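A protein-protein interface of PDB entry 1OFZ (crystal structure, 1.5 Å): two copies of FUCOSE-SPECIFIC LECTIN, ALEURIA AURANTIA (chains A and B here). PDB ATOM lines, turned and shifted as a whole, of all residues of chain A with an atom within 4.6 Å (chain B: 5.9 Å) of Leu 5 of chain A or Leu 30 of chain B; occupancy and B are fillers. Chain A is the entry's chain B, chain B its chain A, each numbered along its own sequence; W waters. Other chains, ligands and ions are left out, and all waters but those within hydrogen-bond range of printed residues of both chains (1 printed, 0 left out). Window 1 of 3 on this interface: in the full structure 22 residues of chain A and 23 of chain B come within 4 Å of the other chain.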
ATOM      1  N   GLU A   3      -6.610 -12.748 -34.425  1.00  0.00           N
ATOM      2  CA  GLU A   3      -5.207 -12.761 -34.769  1.00  0.00           C
ATOM      3  C   GLU A   3      -4.528 -11.449 -34.423  1.00  0.00           C
ATOM      4  O   GLU A   3      -3.410 -11.216 -34.795  1.00  0.00           O
ATOM      5  CB  GLU A   3      -5.061 -13.097 -36.256  1.00  0.00           C
ATOM      6  CG  GLU A   3      -5.619 -14.466 -36.536  1.00  0.00           C
ATOM      7  CD  GLU A   3      -5.611 -14.857 -37.999  1.00  0.00           C
ATOM      8  OE1 GLU A   3      -5.806 -13.993 -38.893  1.00  0.00           O
ATOM      9  OE2 GLU A   3      -5.399 -16.062 -38.252  1.00  0.00           O
ATOM     10  N   PHE A   4      -5.209 -10.598 -33.666  1.00  0.00           N
ATOM     11  CA  PHE A   4      -4.659  -9.310 -33.215  1.00  0.00           C
ATOM     12  C   PHE A   4      -3.671  -9.544 -32.073  1.00  0.00           C
ATOM     13  O   PHE A   4      -4.057 -10.106 -31.049  1.00  0.00           O
ATOM     14  CB  PHE A   4      -5.866  -8.487 -32.760  1.00  0.00           C
ATOM     15  CG  PHE A   4      -5.606  -6.999 -32.456  1.00  0.00           C
ATOM     16  CD1 PHE A   4      -4.415  -6.363 -32.776  1.00  0.00           C
ATOM     17  CD2 PHE A   4      -6.617  -6.260 -31.886  1.00  0.00           C
ATOM     18  CE1 PHE A   4      -4.249  -4.994 -32.497  1.00  0.00           C
ATOM     19  CE2 PHE A   4      -6.478  -4.891 -31.613  1.00  0.00           C
ATOM     20  CZ  PHE A   4      -5.274  -4.269 -31.904  1.00  0.00           C
ATOM     21  N   LEU A   5      -2.413  -9.161 -32.248  1.00  0.00           N
ATOM     22  CA  LEU A   5      -1.411  -9.322 -31.215  1.00  0.00           C
ATOM     23  C   LEU A   5      -1.765  -8.476 -29.985  1.00  0.00           C
ATOM     24  O   LEU A   5      -1.908  -7.261 -30.090  1.00  0.00           O
ATOM     25  CB  LEU A   5      -0.030  -8.933 -31.734  1.00  0.00           C
ATOM     26  CG  LEU A   5       1.168  -9.051 -30.813  1.00  0.00           C
ATOM     27  CD1 LEU A   5       1.469 -10.498 -30.420  1.00  0.00           C
ATOM     28  CD2 LEU A   5       2.339  -8.379 -31.491  1.00  0.00           C
ATOM     29  N   TYR A   6      -1.898  -9.096 -28.823  1.00  0.00           N
ATOM     30  CA  TYR A   6      -2.108  -8.349 -27.579  1.00  0.00           C
ATOM     31  C   TYR A   6      -0.918  -7.459 -27.254  1.00  0.00           C
ATOM     32  O   TYR A   6       0.211  -7.910 -27.222  1.00  0.00           O
ATOM     33  CB  TYR A   6      -2.363  -9.300 -26.421  1.00  0.00           C
ATOM     34  CG  TYR A   6      -2.519  -8.655 -25.087  1.00  0.00           C
ATOM     35  CD1 TYR A   6      -3.480  -7.672 -24.850  1.00  0.00           C
ATOM     36  CD2 TYR A   6      -1.701  -9.000 -24.022  1.00  0.00           C
ATOM     37  CE1 TYR A   6      -3.591  -7.061 -23.613  1.00  0.00           C
ATOM     38  CE2 TYR A   6      -1.830  -8.396 -22.797  1.00  0.00           C
ATOM     39  CZ  TYR A   6      -2.772  -7.427 -22.587  1.00  0.00           C
ATOM     40  OH  TYR A   6      -2.887  -6.866 -21.365  1.00  0.00           O
ATOM     41  N   THR A   7      -1.232  -6.180 -26.985  1.00  0.00           N
ATOM     42  CA  THR A   7      -0.253  -5.089 -26.829  1.00  0.00           C
ATOM     43  C   THR A   7       0.450  -4.668 -28.114  1.00  0.00           C
ATOM     44  O   THR A   7       1.455  -3.980 -28.087  1.00  0.00           O
ATOM     45  CB  THR A   7       0.735  -5.241 -25.647  1.00  0.00           C
ATOM     46  OG1 THR A   7       1.765  -6.213 -25.935  1.00  0.00           O
ATOM     47  CG2 THR A   7       0.010  -5.686 -24.361  1.00  0.00           C
ATOM     48  N   SER A   8      -0.136  -5.042 -29.234  1.00  0.00           N
ATOM     49  CA  SER A   8       0.205  -4.417 -30.506  1.00  0.00           C
ATOM     50  C   SER A   8      -0.002  -2.925 -30.408  1.00  0.00           C
ATOM     51  O   SER A   8      -0.951  -2.443 -29.838  1.00  0.00           O
ATOM     52  CB  SER A   8      -0.687  -4.932 -31.616  1.00  0.00           C
ATOM     53  OG  SER A   8      -0.427  -4.247 -32.864  1.00  0.00           O
ATOM     54  N   GLN A  28      -0.586  -5.067 -35.619  1.00  0.00           N
ATOM     55  CA  GLN A  28       0.264  -6.228 -35.790  1.00  0.00           C
ATOM     56  C   GLN A  28      -0.496  -7.500 -35.467  1.00  0.00           C
ATOM     57  O   GLN A  28      -1.308  -7.551 -34.529  1.00  0.00           O
ATOM     58  CB  GLN A  28       1.509  -6.120 -34.931  1.00  0.00           C
ATOM     59  CG  GLN A  28       2.609  -7.049 -35.303  1.00  0.00           C
ATOM     60  CD  GLN A  28       3.921  -6.618 -34.729  1.00  0.00           C
ATOM     61  OE1 GLN A  28       3.950  -6.151 -33.597  1.00  0.00           O
ATOM     62  NE2 GLN A  28       5.015  -6.781 -35.496  1.00  0.00           N
ATOM     63  N   ASP A  29      -0.215  -8.542 -36.249  1.00  0.00           N
ATOM     64  CA  ASP A  29      -0.803  -9.854 -35.985  1.00  0.00           C
ATOM     65  C   ASP A  29       0.176 -10.750 -35.176  1.00  0.00           C
ATOM     66  O   ASP A  29       1.283 -10.323 -34.820  1.00  0.00           O
ATOM     67  CB  ASP A  29      -1.345 -10.533 -37.248  1.00  0.00           C
ATOM     68  CG  ASP A  29      -0.254 -10.966 -38.226  1.00  0.00           C
ATOM     69  OD1 ASP A  29       0.912 -11.148 -37.840  1.00  0.00           O
ATOM     70  OD2 ASP A  29      -0.493 -11.137 -39.463  1.00  0.00           O
ATOM     71  N   LEU A  30      -0.273 -11.959 -34.858  1.00  0.00           N
ATOM     72  CA  LEU A  30       0.488 -12.879 -34.017  1.00  0.00           C
ATOM     73  C   LEU A  30       1.804 -13.294 -34.667  1.00  0.00           C
ATOM     74  O   LEU A  30       2.768 -13.664 -33.981  1.00  0.00           O
ATOM     75  CB  LEU A  30      -0.349 -14.111 -33.712  1.00  0.00           C
ATOM     76  CG  LEU A  30      -1.671 -13.865 -32.993  1.00  0.00           C
ATOM     77  CD1 LEU A  30      -2.496 -15.113 -32.948  1.00  0.00           C
ATOM     78  CD2 LEU A  30      -1.429 -13.335 -31.608  1.00  0.00           C
ATOM     79  N   LEU A  59       8.147  -8.119 -33.468  1.00  0.00           N
ATOM     80  CA  LEU A  59       6.973  -8.284 -32.640  1.00  0.00           C
ATOM     81  C   LEU A  59       6.930  -7.135 -31.643  1.00  0.00           C
ATOM     82  O   LEU A  59       7.945  -6.756 -31.069  1.00  0.00           O
ATOM     83  CB  LEU A  59       7.030  -9.621 -31.905  1.00  0.00           C
ATOM     84  CG  LEU A  59       6.752 -10.766 -32.861  1.00  0.00           C
ATOM     85  CD1 LEU A  59       7.325 -12.011 -32.279  1.00  0.00           C
ATOM     86  CD2 LEU A  59       5.260 -10.924 -33.178  1.00  0.00           C
ATOM     87  N   PHE A  60       5.725  -6.613 -31.425  1.00  0.00           N
ATOM     88  CA  PHE A  60       5.514  -5.473 -30.538  1.00  0.00           C
ATOM     89  C   PHE A  60       6.185  -4.178 -31.020  1.00  0.00           C
ATOM     90  O   PHE A  60       6.370  -3.245 -30.253  1.00  0.00           O
ATOM     91  CB  PHE A  60       5.863  -5.804 -29.076  1.00  0.00           C
ATOM     92  CG  PHE A  60       5.309  -7.123 -28.625  1.00  0.00           C
ATOM     93  CD1 PHE A  60       4.014  -7.206 -28.226  1.00  0.00           C
ATOM     94  CD2 PHE A  60       6.074  -8.287 -28.709  1.00  0.00           C
ATOM     95  CE1 PHE A  60       3.470  -8.403 -27.873  1.00  0.00           C
ATOM     96  CE2 PHE A  60       5.556  -9.497 -28.328  1.00  0.00           C
ATOM     97  CZ  PHE A  60       4.253  -9.569 -27.915  1.00  0.00           C
ATOM     98  N   GLN A 281      -7.584  -1.363 -27.835  1.00  0.00           N
ATOM     99  CA  GLN A 281      -7.582  -2.826 -27.837  1.00  0.00           C
ATOM    100  C   GLN A 281      -8.305  -3.343 -26.603  1.00  0.00           C
ATOM    101  O   GLN A 281      -8.003  -2.963 -25.484  1.00  0.00           O
ATOM    102  CB  GLN A 281      -6.178  -3.358 -27.927  1.00  0.00           C
ATOM    103  CG  GLN A 281      -6.078  -4.857 -27.989  1.00  0.00           C
ATOM    104  CD  GLN A 281      -4.644  -5.296 -28.190  1.00  0.00           C
ATOM    105  OE1 GLN A 281      -3.785  -5.066 -27.339  1.00  0.00           O
ATOM    106  NE2 GLN A 281      -4.398  -5.994 -29.289  1.00  0.00           N
ATOM    107  N   THR B   2       7.072 -10.890 -24.190  1.00  0.00           N
ATOM    108  CA  THR B   2       7.483 -12.293 -24.288  1.00  0.00           C
ATOM    109  C   THR B   2       6.777 -12.972 -25.466  1.00  0.00           C
ATOM    110  O   THR B   2       5.988 -12.367 -26.195  1.00  0.00           O
ATOM    111  CB  THR B   2       7.145 -13.081 -23.016  1.00  0.00           C
ATOM    112  OG1 THR B   2       5.730 -13.342 -23.014  1.00  0.00           O
ATOM    113  CG2 THR B   2       7.420 -12.278 -21.747  1.00  0.00           C
ATOM    114  N   GLU B   3       7.032 -14.264 -25.617  1.00  0.00           N
ATOM    115  CA  GLU B   3       6.420 -15.049 -26.685  1.00  0.00           C
ATOM    116  C   GLU B   3       5.223 -15.842 -26.164  1.00  0.00           C
ATOM    117  O   GLU B   3       4.694 -16.696 -26.879  1.00  0.00           O
ATOM    118  CB  GLU B   3       7.454 -15.965 -27.324  1.00  0.00           C
ATOM    119  CG  GLU B   3       8.539 -15.132 -27.976  1.00  0.00           C
ATOM    120  CD  GLU B   3       9.739 -15.913 -28.470  1.00  0.00           C
ATOM    121  OE1 GLU B   3      10.125 -16.938 -27.872  1.00  0.00           O
ATOM    122  OE2 GLU B   3      10.306 -15.468 -29.505  1.00  0.00           O
ATOM    123  N   PHE B   4       4.811 -15.586 -24.922  1.00  0.00           N
ATOM    124  CA  PHE B   4       3.626 -16.238 -24.338  1.00  0.00           C
ATOM    125  C   PHE B   4       2.334 -15.692 -24.961  1.00  0.00           C
ATOM    126  O   PHE B   4       2.063 -14.490 -24.869  1.00  0.00           O
ATOM    127  CB  PHE B   4       3.641 -15.956 -22.843  1.00  0.00           C
ATOM    128  CG  PHE B   4       2.671 -16.769 -21.960  1.00  0.00           C
ATOM    129  CD1 PHE B   4       1.877 -17.836 -22.410  1.00  0.00           C
ATOM    130  CD2 PHE B   4       2.609 -16.429 -20.615  1.00  0.00           C
ATOM    131  CE1 PHE B   4       1.059 -18.521 -21.498  1.00  0.00           C
ATOM    132  CE2 PHE B   4       1.806 -17.110 -19.719  1.00  0.00           C
ATOM    133  CZ  PHE B   4       1.033 -18.159 -20.156  1.00  0.00           C
ATOM    134  N   LEU B   5       1.548 -16.551 -25.592  1.00  0.00           N
ATOM    135  CA  LEU B   5       0.291 -16.123 -26.207  1.00  0.00           C
ATOM    136  C   LEU B   5      -0.698 -15.655 -25.146  1.00  0.00           C
ATOM    137  O   LEU B   5      -1.017 -16.392 -24.207  1.00  0.00           O
ATOM    138  CB  LEU B   5      -0.282 -17.274 -27.027  1.00  0.00           C
ATOM    139  CG  LEU B   5      -1.648 -17.032 -27.671  1.00  0.00           C
ATOM    140  CD1 LEU B   5      -1.489 -16.083 -28.832  1.00  0.00           C
ATOM    141  CD2 LEU B   5      -2.218 -18.359 -28.182  1.00  0.00           C
ATOM    142  N   TYR B   6      -1.186 -14.426 -25.278  1.00  0.00           N
ATOM    143  CA  TYR B   6      -2.166 -13.909 -24.333  1.00  0.00           C
ATOM    144  C   TYR B   6      -3.479 -14.679 -24.479  1.00  0.00           C
ATOM    145  O   TYR B   6      -4.012 -14.856 -25.588  1.00  0.00           O
ATOM    146  CB  TYR B   6      -2.405 -12.430 -24.558  1.00  0.00           C
ATOM    147  CG  TYR B   6      -3.544 -11.844 -23.764  1.00  0.00           C
ATOM    148  CD1 TYR B   6      -3.587 -11.940 -22.378  1.00  0.00           C
ATOM    149  CD2 TYR B   6      -4.598 -11.226 -24.390  1.00  0.00           C
ATOM    150  CE1 TYR B   6      -4.633 -11.397 -21.655  1.00  0.00           C
ATOM    151  CE2 TYR B   6      -5.649 -10.682 -23.672  1.00  0.00           C
ATOM    152  CZ  TYR B   6      -5.684 -10.790 -22.315  1.00  0.00           C
ATOM    153  OH  TYR B   6      -6.721 -10.225 -21.576  1.00  0.00           O
ATOM    154  N   GLN B  28       1.110 -22.053 -24.664  1.00  0.00           N
ATOM    155  CA  GLN B  28       1.246 -21.830 -26.088  1.00  0.00           C
ATOM    156  C   GLN B  28       1.983 -20.528 -26.387  1.00  0.00           C
ATOM    157  O   GLN B  28       1.817 -19.515 -25.694  1.00  0.00           O
ATOM    158  CB  GLN B  28      -0.166 -21.797 -26.715  1.00  0.00           C
ATOM    159  CG  GLN B  28      -0.207 -21.959 -28.170  1.00  0.00           C
ATOM    160  CD  GLN B  28      -1.566 -22.403 -28.630  1.00  0.00           C
ATOM    161  OE1 GLN B  28      -2.556 -21.895 -28.143  1.00  0.00           O
ATOM    162  NE2 GLN B  28      -1.607 -23.287 -29.607  1.00  0.00           N
ATOM    163  N   ASP B  29       2.762 -20.551 -27.457  1.00  0.00           N
ATOM    164  CA  ASP B  29       3.454 -19.357 -27.943  1.00  0.00           C
ATOM    165  C   ASP B  29       2.683 -18.690 -29.072  1.00  0.00           C
ATOM    166  O   ASP B  29       1.594 -19.154 -29.456  1.00  0.00           O
ATOM    167  CB  ASP B  29       4.924 -19.637 -28.280  1.00  0.00           C
ATOM    168  CG  ASP B  29       5.132 -20.471 -29.511  1.00  0.00           C
ATOM    169  OD1 ASP B  29       4.260 -20.545 -30.411  1.00  0.00           O
ATOM    170  OD2 ASP B  29       6.221 -21.118 -29.647  1.00  0.00           O
ATOM    171  N   LEU B  30       3.236 -17.572 -29.564  1.00  0.00           N
ATOM    172  CA  LEU B  30       2.552 -16.737 -30.563  1.00  0.00           C
ATOM    173  C   LEU B  30       2.373 -17.463 -31.870  1.00  0.00           C
ATOM    174  O   LEU B  30       1.483 -17.107 -32.639  1.00  0.00           O
ATOM    175  CB  LEU B  30       3.375 -15.457 -30.822  1.00  0.00           C
ATOM    176  CG  LEU B  30       3.525 -14.558 -29.606  1.00  0.00           C
ATOM    177  CD1 LEU B  30       4.438 -13.390 -29.920  1.00  0.00           C
ATOM    178  CD2 LEU B  30       2.207 -14.015 -29.138  1.00  0.00           C
ATOM    179  N   ASN B  31       3.222 -18.461 -32.124  1.00  0.00           N
ATOM    180  CA  ASN B  31       3.150 -19.266 -33.339  1.00  0.00           C
ATOM    181  C   ASN B  31       2.266 -20.499 -33.183  1.00  0.00           C
ATOM    182  O   ASN B  31       2.179 -21.307 -34.121  1.00  0.00           O
ATOM    183  CB  ASN B  31       4.554 -19.729 -33.750  1.00  0.00           C
ATOM    184  CG  ASN B  31       5.482 -18.591 -34.076  1.00  0.00           C
ATOM    185  OD1 ASN B  31       6.679 -18.621 -33.703  1.00  0.00           O
ATOM    186  ND2 ASN B  31       4.967 -17.595 -34.793  1.00  0.00           N
ATOM    187  N   GLY B  32       1.646 -20.678 -32.014  1.00  0.00           N
ATOM    188  CA  GLY B  32       0.755 -21.801 -31.785  1.00  0.00           C
ATOM    189  C   GLY B  32       1.450 -23.070 -31.318  1.00  0.00           C
ATOM    190  O   GLY B  32       0.817 -24.088 -31.100  1.00  0.00           O
ATOM    191  N   LYS B  33       2.753 -23.014 -31.117  1.00  0.00           N
ATOM    192  CA  LYS B  33       3.448 -24.162 -30.575  1.00  0.00           C
ATOM    193  C   LYS B  33       3.184 -24.290 -29.086  1.00  0.00           C
ATOM    194  O   LYS B  33       2.939 -23.297 -28.400  1.00  0.00           O
ATOM    195  CB  LYS B  33       4.945 -24.048 -30.808  1.00  0.00           C
ATOM    196  CG  LYS B  33       5.314 -23.843 -32.273  1.00  0.00           C
ATOM    197  CD  LYS B  33       4.826 -24.953 -33.140  1.00  0.00           C
ATOM    198  CE  LYS B  33       5.211 -24.735 -34.628  1.00  0.00           C
ATOM    199  NZ  LYS B  33       4.758 -25.908 -35.438  1.00  0.00           N
ATOM    200  N   ARG B  35       4.918 -25.065 -25.742  1.00  0.00           N
ATOM    201  CA  ARG B  35       6.241 -25.066 -25.107  1.00  0.00           C
ATOM    202  C   ARG B  35       6.170 -25.633 -23.705  1.00  0.00           C
ATOM    203  O   ARG B  35       5.121 -25.645 -23.058  1.00  0.00           O
ATOM    204  CB  ARG B  35       6.799 -23.659 -25.028  1.00  0.00           C
ATOM    205  CG  ARG B  35       7.100 -23.046 -26.370  1.00  0.00           C
ATOM    206  CD  ARG B  35       7.666 -21.668 -26.184  1.00  0.00           C
ATOM    207  NE  ARG B  35       7.874 -21.008 -27.463  1.00  0.00           N
ATOM    208  CZ  ARG B  35       8.553 -19.858 -27.595  1.00  0.00           C
ATOM    209  NH1 ARG B  35       9.086 -19.245 -26.539  1.00  0.00           N
ATOM    210  NH2 ARG B  35       8.661 -19.341 -28.801  1.00  0.00           N
ATOM    211  N   LEU B  59      -4.354 -22.252 -32.383  1.00  0.00           N
ATOM    212  CA  LEU B  59      -4.169 -21.107 -31.509  1.00  0.00           C
ATOM    213  C   LEU B  59      -5.311 -21.021 -30.520  1.00  0.00           C
ATOM    214  O   LEU B  59      -6.479 -21.155 -30.888  1.00  0.00           O
ATOM    215  CB  LEU B  59      -4.009 -19.817 -32.311  1.00  0.00           C
ATOM    216  CG  LEU B  59      -2.615 -19.682 -32.931  1.00  0.00           C
ATOM    217  CD1 LEU B  59      -2.684 -18.736 -34.137  1.00  0.00           C
ATOM    218  CD2 LEU B  59      -1.643 -19.183 -31.871  1.00  0.00           C
HETATM  219  O   HOH W   1       5.122 -14.979 -34.171  1.00  0.00           O
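Leu 5 of chain A touches just one residue of chain B: Leu 30 (3.8 Å).
Of the printed residues of chain A, Leu 30 of chain B touches Leu 5 (3.8 Å), Leu 30 (3.7 Å) and Leu 59 (3.98 Å).
Of the printed residues of chain A, Tyr 6 of chain B touches Tyr 6 (3.4 Å).
Of the printed residues of chain A, Leu 59 of chain B touches Leu 30.
Of the printed residues of chain A, Leu 5 of chain B touches Leu 30 (3.9 Å).
Of the printed residues of chain B, Leu 59 of chain A touches Leu 30.
Gln 28 of chain A touches none of the printed residues of chain B.
The nearest printed residue of chain B that does not touch Leu 5 of chain A is Thr 2 of chain B (6.5 Å).
The nearest printed residue of chain A that does not touch Leu 30 of chain B is Phe 60 of chain A (4.3 Å).
Leu 5 of chain A touches Leu 30 of chain B, and with the chains exchanged Leu 30 of chain A touches Leu 5 of chain B.
Tyr 6 of chain A touches its own counterpart, Tyr 6 of chain B.
Leu 30 of chain A touches its own counterpart, Leu 30 of chain B.
Leu 30 of chain A touches Leu 59 of chain B, and with the chains exchanged Leu 59 of chain A touches Leu 30 of chain B.
Printed residues of chain A that touch a printed residue of chain B: Leu 5, Tyr 6, Leu 30, Leu 59 and Phe 60.
Hydrophobic or aromatic side chains of chain B within 4 Å of the printed part of chain A: Leu 5, Tyr 6, Leu 30 and Leu 59.
Among the printed residues, 7 pairs touch across the chains.
Among the printed residues, no Asp or Glu carboxylate lies within 4 Å of a Lys or Arg side-chain nitrogen of the other chain.
The backbone NH (N) of Leu 5 of chain A is in hydrogen-bond range of the backbone carbonyl oxygen (O) of Gln 28 of chain A.
O of Leu 5 of chain A is in hydrogen-bond range of NE2 of Gln 281 of chain A.
The side-chain amide oxygen (OE1) of Gln 28 of chain A sits at hydrogen-bond distance from the backbone NH (N) of Phe 60 of chain A (2.8 Å).
OG1 of Thr 2 of chain B lies within hydrogen-bond range of N of Phe 4 of chain B.
The backbone carbonyl oxygen (O) of Glu 3 of chain A lies within hydrogen-bond range of the backbone NH (N) of Leu 30 of chain A (3.2 Å).
The backbone NH of Leu 5 of chain B lies within hydrogen-bond range of the backbone carbonyl oxygen of Gln 28 of chain B (3.0 Å).
Among the printed residues, merely in contact across the chains: Leu 5 of chain A with Leu 30 of chain B (3.8 Å), Tyr 6 of chain A with Tyr 6 of chain B (3.4 Å), Leu 30 of chain A with Leu 5 of chain B (3.9 Å), Leu 30 of chain A with Leu 30 of chain B (3.7 Å), Leu 30 of chain A with Leu 59 of chain B (3.8 Å), Leu 59 of chain A with Leu 30 of chain B (3.98 Å) and Phe 60 of chain A with Thr 2 of chain B (3.6 Å).
Water W1 bridges the side-chain amide nitrogen of Asn 31 of chain B (2.7 Å) and the backbone carbonyl oxygen of Leu 30 of chain A (2.7 Å).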
